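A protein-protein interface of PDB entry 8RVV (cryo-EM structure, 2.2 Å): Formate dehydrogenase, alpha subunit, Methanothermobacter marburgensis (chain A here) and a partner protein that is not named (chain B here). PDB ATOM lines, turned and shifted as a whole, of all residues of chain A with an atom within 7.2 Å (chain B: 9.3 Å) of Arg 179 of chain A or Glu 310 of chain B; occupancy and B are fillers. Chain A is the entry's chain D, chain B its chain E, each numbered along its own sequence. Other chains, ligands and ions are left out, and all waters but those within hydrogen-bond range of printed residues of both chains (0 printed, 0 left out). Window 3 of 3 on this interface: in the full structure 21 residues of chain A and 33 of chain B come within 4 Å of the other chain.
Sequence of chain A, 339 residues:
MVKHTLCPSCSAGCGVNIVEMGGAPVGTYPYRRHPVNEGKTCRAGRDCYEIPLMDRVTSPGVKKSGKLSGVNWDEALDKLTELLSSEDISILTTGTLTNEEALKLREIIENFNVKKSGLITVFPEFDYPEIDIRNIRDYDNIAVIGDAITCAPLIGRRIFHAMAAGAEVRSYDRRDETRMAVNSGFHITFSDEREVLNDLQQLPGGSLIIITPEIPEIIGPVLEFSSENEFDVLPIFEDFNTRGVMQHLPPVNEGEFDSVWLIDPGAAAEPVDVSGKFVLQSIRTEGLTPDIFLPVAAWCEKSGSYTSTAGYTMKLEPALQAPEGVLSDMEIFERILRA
The backbone carbonyl oxygen (O) of Ile 281 of chain B lies within hydrogen-bond range of the guanidinium group (NH2) of Arg 179 of chain A (3.5 Å).
NH1 of Arg 179 of chain A is in salt-bridge range of OE2 of Glu 310 of chain B (3.7 Å).
O of Met 342 of chain B is in hydrogen-bond range of NH1 of Arg 279 of chain B (2.8 Å).
NZ of Lys 311 of chain B is in salt-bridge range of OD2 of Asp 309 of chain B (2.7 Å).
The side-chain carboxylate (OE2) of Glu 307 of chain B is in salt-bridge range of the side-chain amino group (NZ) of Lys 311 of chain B.
OG1 of Thr 150 of chain A lies within hydrogen-bond range of OD2 of Asp 147 of chain A (2.4 Å).
The side-chain amide nitrogen of Asn 183 of chain A is in hydrogen-bond range of the backbone carbonyl oxygen of Arg 179 of chain A (3.0 Å).
OD2 of Asp 147 of chain A is in hydrogen-bond range of N of Arg 179 of chain A (3.4 Å).
OE2 of Glu 310 of chain B touches CG2 of Thr 150 of chain A, 3.4 Å away.
O of Pro 153 of chain A touches CE of Met 342 of chain B, 3.8 Å away.
Phe 160 of chain A touches Arg 279 of chain B.
Phe 160 of chain A touches Met 342 of chain B.
N of Lys 311 of chain B touches NH2 of Arg 179 of chain A, at 3.7 Å.
OD1 of Asn 183 of chain A touches O of Lys 278 of chain B, 3.8 Å away.
Ile 149 of chain A touches none of the printed residues of chain B.
Printed residues of chain B within 4 Å of Thr 150 of chain A: Glu 310 (3.4 Å).
No residue of chain B comes within 4 Å of Ala 181 of chain A.
No residue of chain B comes within 4 Å of Val 182 of chain A.
Printed residues of chain A within 4 Å of Arg 279 of chain B: Phe 160.
Of the printed residues of chain A, Ile 281 of chain B touches Arg 179 (3.5 Å).
Asp 309 of chain B touches none of the printed residues of chain A.
Of chain A, only Thr 150 and Arg 179 come within 4 Å of Glu 310 of chain B.
The nearest residue of chain B that does not touch Arg 179 of chain A is Asp 309 of chain B (4.5 Å).
The nearest printed residue of chain A that does not touch Lys 311 of chain B is Glu 177 of chain A (5.2 Å).
Hydrophobic or aromatic side chains of chain A within 4 Å of the printed part of chain B: Phe 160.
Of the 16 printed residues of chain B, 6 touch a printed residue of chain A.
Along chain B the printed residues that touch a printed residue of chain A span positions 278 to 342.
Among the printed residues, 8 pairs touch across the chains.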
ATOM      1  N   ASP A 147      35.741 -24.346  27.480  1.00  0.00           N
ATOM      2  CA  ASP A 147      34.611 -23.455  27.216  1.00  0.00           C
ATOM      3  C   ASP A 147      33.320 -24.208  27.510  1.00  0.00           C
ATOM      4  O   ASP A 147      32.750 -24.877  26.648  1.00  0.00           O
ATOM      5  CB  ASP A 147      34.656 -22.952  25.780  1.00  0.00           C
ATOM      6  CG  ASP A 147      33.611 -21.892  25.499  1.00  0.00           C
ATOM      7  OD1 ASP A 147      32.802 -21.595  26.401  1.00  0.00           O
ATOM      8  OD2 ASP A 147      33.598 -21.358  24.373  1.00  0.00           O
ATOM      9  N   ALA A 148      32.851 -24.089  28.752  1.00  0.00           N
ATOM     10  CA  ALA A 148      31.684 -24.852  29.177  1.00  0.00           C
ATOM     11  C   ALA A 148      30.405 -24.318  28.544  1.00  0.00           C
ATOM     12  O   ALA A 148      29.478 -25.088  28.274  1.00  0.00           O
ATOM     13  CB  ALA A 148      31.575 -24.832  30.699  1.00  0.00           C
ATOM     14  N   ILE A 149      30.328 -23.007  28.313  1.00  0.00           N
ATOM     15  CA  ILE A 149      29.116 -22.430  27.732  1.00  0.00           C
ATOM     16  C   ILE A 149      28.888 -22.981  26.330  1.00  0.00           C
ATOM     17  O   ILE A 149      27.775 -23.383  25.975  1.00  0.00           O
ATOM     18  CB  ILE A 149      29.196 -20.894  27.725  1.00  0.00           C
ATOM     19  CG1 ILE A 149      29.176 -20.346  29.153  1.00  0.00           C
ATOM     20  CG2 ILE A 149      28.040 -20.310  26.931  1.00  0.00           C
ATOM     21  CD1 ILE A 149      29.759 -18.960  29.282  1.00  0.00           C
ATOM     22  N   THR A 150      29.937 -23.004  25.509  1.00  0.00           N
ATOM     23  CA  THR A 150      29.797 -23.516  24.151  1.00  0.00           C
ATOM     24  C   THR A 150      29.541 -25.018  24.149  1.00  0.00           C
ATOM     25  O   THR A 150      28.726 -25.511  23.364  1.00  0.00           O
ATOM     26  CB  THR A 150      31.043 -23.183  23.335  1.00  0.00           C
ATOM     27  OG1 THR A 150      31.383 -21.805  23.524  1.00  0.00           O
ATOM     28  CG2 THR A 150      30.804 -23.441  21.861  1.00  0.00           C
ATOM     29  N   CYS A 151      30.230 -25.761  25.016  1.00  0.00           N
ATOM     30  CA  CYS A 151      30.039 -27.206  25.065  1.00  0.00           C
ATOM     31  C   CYS A 151      28.617 -27.566  25.479  1.00  0.00           C
ATOM     32  O   CYS A 151      28.003 -28.466  24.898  1.00  0.00           O
ATOM     33  CB  CYS A 151      31.051 -27.835  26.021  1.00  0.00           C
ATOM     34  SG  CYS A 151      32.730 -27.892  25.368  1.00  0.00           S
ATOM     35  N   PRO A 153      25.423 -25.123  26.464  1.00  0.00           N
ATOM     36  CA  PRO A 153      24.867 -23.803  26.800  1.00  0.00           C
ATOM     37  C   PRO A 153      23.972 -23.794  28.028  1.00  0.00           C
ATOM     38  O   PRO A 153      23.980 -22.814  28.783  1.00  0.00           O
ATOM     39  CB  PRO A 153      24.091 -23.435  25.532  1.00  0.00           C
ATOM     40  CG  PRO A 153      24.836 -24.103  24.446  1.00  0.00           C
ATOM     41  CD  PRO A 153      25.371 -25.384  25.015  1.00  0.00           C
ATOM     42  N   PHE A 160      26.125 -18.918  34.906  1.00  0.00           N
ATOM     43  CA  PHE A 160      25.722 -17.517  35.013  1.00  0.00           C
ATOM     44  C   PHE A 160      24.872 -17.282  36.257  1.00  0.00           C
ATOM     45  O   PHE A 160      25.025 -16.261  36.941  1.00  0.00           O
ATOM     46  CB  PHE A 160      24.953 -17.093  33.761  1.00  0.00           C
ATOM     47  CG  PHE A 160      25.833 -16.633  32.640  1.00  0.00           C
ATOM     48  CD1 PHE A 160      26.537 -15.448  32.736  1.00  0.00           C
ATOM     49  CD2 PHE A 160      25.952 -17.384  31.487  1.00  0.00           C
ATOM     50  CE1 PHE A 160      27.348 -15.026  31.708  1.00  0.00           C
ATOM     51  CE2 PHE A 160      26.761 -16.967  30.457  1.00  0.00           C
ATOM     52  CZ  PHE A 160      27.456 -15.786  30.565  1.00  0.00           C
ATOM     53  N   SER A 171      38.204 -19.511  35.010  1.00  0.00           N
ATOM     54  CA  SER A 171      38.187 -20.303  33.791  1.00  0.00           C
ATOM     55  C   SER A 171      39.605 -20.499  33.279  1.00  0.00           C
ATOM     56  O   SER A 171      40.434 -19.589  33.335  1.00  0.00           O
ATOM     57  CB  SER A 171      37.330 -19.644  32.702  1.00  0.00           C
ATOM     58  OG  SER A 171      37.740 -18.315  32.450  1.00  0.00           O
ATOM     59  N   ARG A 175      42.847 -20.902  25.025  1.00  0.00           N
ATOM     60  CA  ARG A 175      42.411 -19.745  24.265  1.00  0.00           C
ATOM     61  C   ARG A 175      41.927 -18.678  25.237  1.00  0.00           C
ATOM     62  O   ARG A 175      41.546 -18.976  26.372  1.00  0.00           O
ATOM     63  CB  ARG A 175      41.301 -20.118  23.280  1.00  0.00           C
ATOM     64  CG  ARG A 175      41.755 -21.067  22.185  1.00  0.00           C
ATOM     65  CD  ARG A 175      40.606 -21.887  21.632  1.00  0.00           C
ATOM     66  NE  ARG A 175      39.991 -22.733  22.649  1.00  0.00           N
ATOM     67  CZ  ARG A 175      38.695 -23.001  22.731  1.00  0.00           C
ATOM     68  NH1 ARG A 175      37.829 -22.521  21.852  1.00  0.00           N
ATOM     69  NH2 ARG A 175      38.253 -23.778  23.716  1.00  0.00           N
ATOM     70  N   GLU A 177      39.615 -16.024  24.318  1.00  0.00           N
ATOM     71  CA  GLU A 177      38.445 -15.298  23.845  1.00  0.00           C
ATOM     72  C   GLU A 177      37.198 -16.174  23.777  1.00  0.00           C
ATOM     73  O   GLU A 177      36.198 -15.758  23.181  1.00  0.00           O
ATOM     74  CB  GLU A 177      38.731 -14.656  22.478  1.00  0.00           C
ATOM     75  CG  GLU A 177      38.584 -15.571  21.266  1.00  0.00           C
ATOM     76  CD  GLU A 177      39.784 -16.469  21.066  1.00  0.00           C
ATOM     77  OE1 GLU A 177      40.347 -16.942  22.076  1.00  0.00           O
ATOM     78  OE2 GLU A 177      40.164 -16.703  19.900  1.00  0.00           O
ATOM     79  N   THR A 178      37.225 -17.359  24.376  1.00  0.00           N
ATOM     80  CA  THR A 178      36.044 -18.200  24.416  1.00  0.00           C
ATOM     81  C   THR A 178      34.945 -17.520  25.232  1.00  0.00           C
ATOM     82  O   THR A 178      35.157 -16.489  25.875  1.00  0.00           O
ATOM     83  CB  THR A 178      36.382 -19.567  25.008  1.00  0.00           C
ATOM     84  OG1 THR A 178      36.827 -19.409  26.361  1.00  0.00           O
ATOM     85  CG2 THR A 178      37.470 -20.248  24.196  1.00  0.00           C
ATOM     86  N   ARG A 179      33.748 -18.110  25.194  1.00  0.00           N
ATOM     87  CA  ARG A 179      32.624 -17.527  25.918  1.00  0.00           C
ATOM     88  C   ARG A 179      32.889 -17.498  27.416  1.00  0.00           C
ATOM     89  O   ARG A 179      32.610 -16.496  28.085  1.00  0.00           O
ATOM     90  CB  ARG A 179      31.344 -18.306  25.618  1.00  0.00           C
ATOM     91  CG  ARG A 179      30.827 -18.134  24.202  1.00  0.00           C
ATOM     92  CD  ARG A 179      29.367 -18.529  24.086  1.00  0.00           C
ATOM     93  NE  ARG A 179      28.742 -17.965  22.896  1.00  0.00           N
ATOM     94  CZ  ARG A 179      28.736 -18.541  21.701  1.00  0.00           C
ATOM     95  NH1 ARG A 179      29.304 -19.717  21.494  1.00  0.00           N
ATOM     96  NH2 ARG A 179      28.147 -17.917  20.685  1.00  0.00           N
ATOM     97  N   MET A 180      33.426 -18.591  27.964  1.00  0.00           N
ATOM     98  CA  MET A 180      33.775 -18.603  29.379  1.00  0.00           C
ATOM     99  C   MET A 180      34.857 -17.576  29.679  1.00  0.00           C
ATOM    100  O   MET A 180      34.783 -16.860  30.684  1.00  0.00           O
ATOM    101  CB  MET A 180      34.234 -20.002  29.796  1.00  0.00           C
ATOM    102  CG  MET A 180      33.104 -20.929  30.235  1.00  0.00           C
ATOM    103  SD  MET A 180      32.147 -20.363  31.657  1.00  0.00           S
ATOM    104  CE  MET A 180      33.415 -19.639  32.687  1.00  0.00           C
ATOM    105  N   ALA A 181      35.863 -17.477  28.810  1.00  0.00           N
ATOM    106  CA  ALA A 181      36.917 -16.489  29.009  1.00  0.00           C
ATOM    107  C   ALA A 181      36.340 -15.083  29.087  1.00  0.00           C
ATOM    108  O   ALA A 181      36.783 -14.266  29.901  1.00  0.00           O
ATOM    109  CB  ALA A 181      37.943 -16.584  27.882  1.00  0.00           C
ATOM    110  N   VAL A 182      35.357 -14.783  28.239  1.00  0.00           N
ATOM    111  CA  VAL A 182      34.758 -13.454  28.233  1.00  0.00           C
ATOM    112  C   VAL A 182      33.912 -13.236  29.480  1.00  0.00           C
ATOM    113  O   VAL A 182      33.953 -12.162  30.091  1.00  0.00           O
ATOM    114  CB  VAL A 182      33.933 -13.256  26.951  1.00  0.00           C
ATOM    115  CG1 VAL A 182      33.088 -12.000  27.050  1.00  0.00           C
ATOM    116  CG2 VAL A 182      34.848 -13.196  25.743  1.00  0.00           C
ATOM    117  N   ASN A 183      33.129 -14.236  29.874  1.00  0.00           N
ATOM    118  CA  ASN A 183      32.133 -14.066  30.924  1.00  0.00           C
ATOM    119  C   ASN A 183      32.596 -14.550  32.291  1.00  0.00           C
ATOM    120  O   ASN A 183      31.833 -14.451  33.254  1.00  0.00           O
ATOM    121  CB  ASN A 183      30.844 -14.794  30.536  1.00  0.00           C
ATOM    122  CG  ASN A 183      30.094 -14.090  29.427  1.00  0.00           C
ATOM    123  OD1 ASN A 183      29.380 -13.119  29.667  1.00  0.00           O
ATOM    124  ND2 ASN A 183      30.253 -14.577  28.203  1.00  0.00           N
ATOM    125  N   SER A 184      33.816 -15.066  32.405  1.00  0.00           N
ATOM    126  CA  SER A 184      34.306 -15.566  33.681  1.00  0.00           C
ATOM    127  C   SER A 184      34.729 -14.421  34.591  1.00  0.00           C
ATOM    128  O   SER A 184      35.042 -13.317  34.136  1.00  0.00           O
ATOM    129  CB  SER A 184      35.487 -16.514  33.474  1.00  0.00           C
ATOM    130  OG  SER A 184      36.424 -15.979  32.559  1.00  0.00           O
ATOM    131  N   TRP B 277      23.234  -8.113  27.381  1.00  0.00           N
ATOM    132  CA  TRP B 277      23.564  -8.396  25.989  1.00  0.00           C
ATOM    133  C   TRP B 277      24.888  -9.131  25.876  1.00  0.00           C
ATOM    134  O   TRP B 277      25.101  -9.879  24.917  1.00  0.00           O
ATOM    135  CB  TRP B 277      23.612  -7.097  25.177  1.00  0.00           C
ATOM    136  CG  TRP B 277      22.310  -6.329  25.111  1.00  0.00           C
ATOM    137  CD1 TRP B 277      22.146  -4.989  25.290  1.00  0.00           C
ATOM    138  CD2 TRP B 277      21.003  -6.857  24.837  1.00  0.00           C
ATOM    139  NE1 TRP B 277      20.826  -4.648  25.152  1.00  0.00           N
ATOM    140  CE2 TRP B 277      20.102  -5.775  24.873  1.00  0.00           C
ATOM    141  CE3 TRP B 277      20.508  -8.133  24.563  1.00  0.00           C
ATOM    142  CZ2 TRP B 277      18.738  -5.932  24.647  1.00  0.00           C
ATOM    143  CZ3 TRP B 277      19.154  -8.285  24.343  1.00  0.00           C
ATOM    144  CH2 TRP B 277      18.285  -7.192  24.386  1.00  0.00           C
ATOM    145  N   LYS B 278      25.787  -8.933  26.842  1.00  0.00           N
ATOM    146  CA  LYS B 278      27.047  -9.664  26.845  1.00  0.00           C
ATOM    147  C   LYS B 278      26.843 -11.172  26.908  1.00  0.00           C
ATOM    148  O   LYS B 278      27.735 -11.925  26.511  1.00  0.00           O
ATOM    149  CB  LYS B 278      27.897  -9.209  28.029  1.00  0.00           C
ATOM    150  CG  LYS B 278      29.396  -9.339  27.808  1.00  0.00           C
ATOM    151  CD  LYS B 278      30.220  -8.861  29.005  1.00  0.00           C
ATOM    152  CE  LYS B 278      29.530  -9.094  30.342  1.00  0.00           C
ATOM    153  NZ  LYS B 278      30.452  -8.869  31.489  1.00  0.00           N
ATOM    154  N   ARG B 279      25.690 -11.626  27.406  1.00  0.00           N
ATOM    155  CA  ARG B 279      25.432 -13.052  27.572  1.00  0.00           C
ATOM    156  C   ARG B 279      25.041 -13.740  26.273  1.00  0.00           C
ATOM    157  O   ARG B 279      25.346 -14.922  26.094  1.00  0.00           O
ATOM    158  CB  ARG B 279      24.310 -13.263  28.586  1.00  0.00           C
ATOM    159  CG  ARG B 279      24.724 -13.184  30.023  1.00  0.00           C
ATOM    160  CD  ARG B 279      23.612 -13.692  30.909  1.00  0.00           C
ATOM    161  NE  ARG B 279      23.540 -12.974  32.173  1.00  0.00           N
ATOM    162  CZ  ARG B 279      22.454 -12.894  32.929  1.00  0.00           C
ATOM    163  NH1 ARG B 279      21.318 -13.469  32.572  1.00  0.00           N
ATOM    164  NH2 ARG B 279      22.511 -12.222  34.074  1.00  0.00           N
ATOM    165  N   CYS B 280      24.367 -13.030  25.373  1.00  0.00           N
ATOM    166  CA  CYS B 280      23.646 -13.664  24.276  1.00  0.00           C
ATOM    167  C   CYS B 280      24.531 -14.647  23.518  1.00  0.00           C
ATOM    168  O   CYS B 280      25.662 -14.328  23.148  1.00  0.00           O
ATOM    169  CB  CYS B 280      23.105 -12.591  23.330  1.00  0.00           C
ATOM    170  SG  CYS B 280      22.291 -13.222  21.852  1.00  0.00           S
ATOM    171  N   ILE B 281      24.006 -15.852  23.297  1.00  0.00           N
ATOM    172  CA  ILE B 281      24.731 -16.903  22.593  1.00  0.00           C
ATOM    173  C   ILE B 281      24.277 -17.036  21.143  1.00  0.00           C
ATOM    174  O   ILE B 281      24.690 -17.969  20.454  1.00  0.00           O
ATOM    175  CB  ILE B 281      24.608 -18.251  23.326  1.00  0.00           C
ATOM    176  CG1 ILE B 281      23.142 -18.594  23.594  1.00  0.00           C
ATOM    177  CG2 ILE B 281      25.380 -18.217  24.631  1.00  0.00           C
ATOM    178  CD1 ILE B 281      22.856 -20.075  23.569  1.00  0.00           C
ATOM    179  N   ASN B 282      23.426 -16.127  20.667  1.00  0.00           N
ATOM    180  CA  ASN B 282      23.049 -16.080  19.255  1.00  0.00           C
ATOM    181  C   ASN B 282      22.322 -17.355  18.828  1.00  0.00           C
ATOM    182  O   ASN B 282      22.498 -17.850  17.715  1.00  0.00           O
ATOM    183  CB  ASN B 282      24.283 -15.840  18.385  1.00  0.00           C
ATOM    184  CG  ASN B 282      23.959 -15.141  17.089  1.00  0.00           C
ATOM    185  OD1 ASN B 282      23.227 -14.153  17.068  1.00  0.00           O
ATOM    186  ND2 ASN B 282      24.513 -15.642  15.994  1.00  0.00           N
ATOM    187  N   CYS B 283      21.492 -17.889  19.721  1.00  0.00           N
ATOM    188  CA  CYS B 283      20.797 -19.143  19.467  1.00  0.00           C
ATOM    189  C   CYS B 283      19.505 -18.970  18.686  1.00  0.00           C
ATOM    190  O   CYS B 283      18.982 -19.957  18.162  1.00  0.00           O
ATOM    191  CB  CYS B 283      20.489 -19.842  20.793  1.00  0.00           C
ATOM    192  SG  CYS B 283      19.171 -19.077  21.744  1.00  0.00           S
ATOM    193  N   LEU B 306      24.682 -11.553  10.497  1.00  0.00           N
ATOM    194  CA  LEU B 306      24.930 -12.662  11.407  1.00  0.00           C
ATOM    195  C   LEU B 306      26.320 -12.559  12.011  1.00  0.00           C
ATOM    196  O   LEU B 306      27.304 -12.295  11.316  1.00  0.00           O
ATOM    197  CB  LEU B 306      24.773 -13.995  10.677  1.00  0.00           C
ATOM    198  CG  LEU B 306      25.024 -15.261  11.501  1.00  0.00           C
ATOM    199  CD1 LEU B 306      23.927 -15.471  12.523  1.00  0.00           C
ATOM    200  CD2 LEU B 306      25.138 -16.468  10.590  1.00  0.00           C
ATOM    201  N   GLU B 307      26.393 -12.772  13.318  1.00  0.00           N
ATOM    202  CA  GLU B 307      27.664 -12.801  14.027  1.00  0.00           C
ATOM    203  C   GLU B 307      28.273 -14.189  13.873  1.00  0.00           C
ATOM    204  O   GLU B 307      27.739 -15.172  14.395  1.00  0.00           O
ATOM    205  CB  GLU B 307      27.455 -12.438  15.492  1.00  0.00           C
ATOM    206  CG  GLU B 307      28.586 -11.633  16.073  1.00  0.00           C
ATOM    207  CD  GLU B 307      29.604 -12.502  16.751  1.00  0.00           C
ATOM    208  OE1 GLU B 307      29.218 -13.265  17.657  1.00  0.00           O
ATOM    209  OE2 GLU B 307      30.788 -12.428  16.369  1.00  0.00           O
ATOM    210  N   SER B 308      29.389 -14.272  13.152  1.00  0.00           N
ATOM    211  CA  SER B 308      29.974 -15.552  12.778  1.00  0.00           C
ATOM    212  C   SER B 308      30.964 -16.090  13.801  1.00  0.00           C
ATOM    213  O   SER B 308      31.422 -17.228  13.650  1.00  0.00           O
ATOM    214  CB  SER B 308      30.666 -15.427  11.419  1.00  0.00           C
ATOM    215  OG  SER B 308      31.284 -14.160  11.283  1.00  0.00           O
ATOM    216  N   ASP B 309      31.308 -15.319  14.824  1.00  0.00           N
ATOM    217  CA  ASP B 309      32.220 -15.771  15.863  1.00  0.00           C
ATOM    218  C   ASP B 309      31.438 -16.294  17.060  1.00  0.00           C
ATOM    219  O   ASP B 309      30.256 -15.991  17.242  1.00  0.00           O
ATOM    220  CB  ASP B 309      33.151 -14.639  16.304  1.00  0.00           C
ATOM    221  CG  ASP B 309      34.103 -14.209  15.209  1.00  0.00           C
ATOM    222  OD1 ASP B 309      34.369 -15.019  14.296  1.00  0.00           O
ATOM    223  OD2 ASP B 309      34.587 -13.059  15.260  1.00  0.00           O
ATOM    224  N   GLU B 310      32.117 -17.088  17.880  1.00  0.00           N
ATOM    225  CA  GLU B 310      31.505 -17.666  19.074  1.00  0.00           C
ATOM    226  C   GLU B 310      31.627 -16.675  20.232  1.00  0.00           C
ATOM    227  O   GLU B 310      32.320 -16.895  21.225  1.00  0.00           O
ATOM    228  CB  GLU B 310      32.147 -19.007  19.405  1.00  0.00           C
ATOM    229  CG  GLU B 310      32.093 -20.016  18.269  1.00  0.00           C
ATOM    230  CD  GLU B 310      30.805 -20.817  18.252  1.00  0.00           C
ATOM    231  OE1 GLU B 310      29.822 -20.356  17.634  1.00  0.00           O
ATOM    232  OE2 GLU B 310      30.775 -21.911  18.852  1.00  0.00           O
ATOM    233  N   LYS B 311      30.925 -15.555  20.077  1.00  0.00           N
ATOM    234  CA  LYS B 311      30.883 -14.519  21.098  1.00  0.00           C
ATOM    235  C   LYS B 311      29.535 -13.820  21.023  1.00  0.00           C
ATOM    236  O   LYS B 311      28.770 -14.003  20.076  1.00  0.00           O
ATOM    237  CB  LYS B 311      32.030 -13.516  20.929  1.00  0.00           C
ATOM    238  CG  LYS B 311      32.155 -12.936  19.534  1.00  0.00           C
ATOM    239  CD  LYS B 311      32.601 -11.487  19.593  1.00  0.00           C
ATOM    240  CE  LYS B 311      32.927 -10.928  18.219  1.00  0.00           C
ATOM    241  NZ  LYS B 311      33.952 -11.726  17.496  1.00  0.00           N
ATOM    242  N   ALA B 312      29.251 -13.016  22.038  1.00  0.00           N
ATOM    243  CA  ALA B 312      27.970 -12.331  22.102  1.00  0.00           C
ATOM    244  C   ALA B 312      27.814 -11.405  20.901  1.00  0.00           C
ATOM    245  O   ALA B 312      28.747 -10.659  20.576  1.00  0.00           O
ATOM    246  CB  ALA B 312      27.851 -11.535  23.398  1.00  0.00           C
ATOM    247  N   PRO B 313      26.674 -11.420  20.216  1.00  0.00           N
ATOM    248  CA  PRO B 313      26.494 -10.519  19.076  1.00  0.00           C
ATOM    249  C   PRO B 313      26.305  -9.079  19.517  1.00  0.00           C
ATOM    250  O   PRO B 313      25.889  -8.786  20.639  1.00  0.00           O
ATOM    251  CB  PRO B 313      25.236 -11.058  18.392  1.00  0.00           C
ATOM    252  CG  PRO B 313      24.479 -11.707  19.472  1.00  0.00           C
ATOM    253  CD  PRO B 313      25.501 -12.291  20.407  1.00  0.00           C
ATOM    254  N   MET B 342      19.749 -17.656  28.040  1.00  0.00           N
ATOM    255  CA  MET B 342      20.627 -16.788  28.809  1.00  0.00           C
ATOM    256  C   MET B 342      19.872 -15.889  29.780  1.00  0.00           C
ATOM    257  O   MET B 342      20.500 -15.077  30.462  1.00  0.00           O
ATOM    258  CB  MET B 342      21.464 -15.936  27.845  1.00  0.00           C
ATOM    259  CG  MET B 342      22.797 -16.545  27.405  1.00  0.00           C
ATOM    260  SD  MET B 342      23.661 -17.580  28.607  1.00  0.00           S
ATOM    261  CE  MET B 342      23.581 -19.189  27.830  1.00  0.00           C
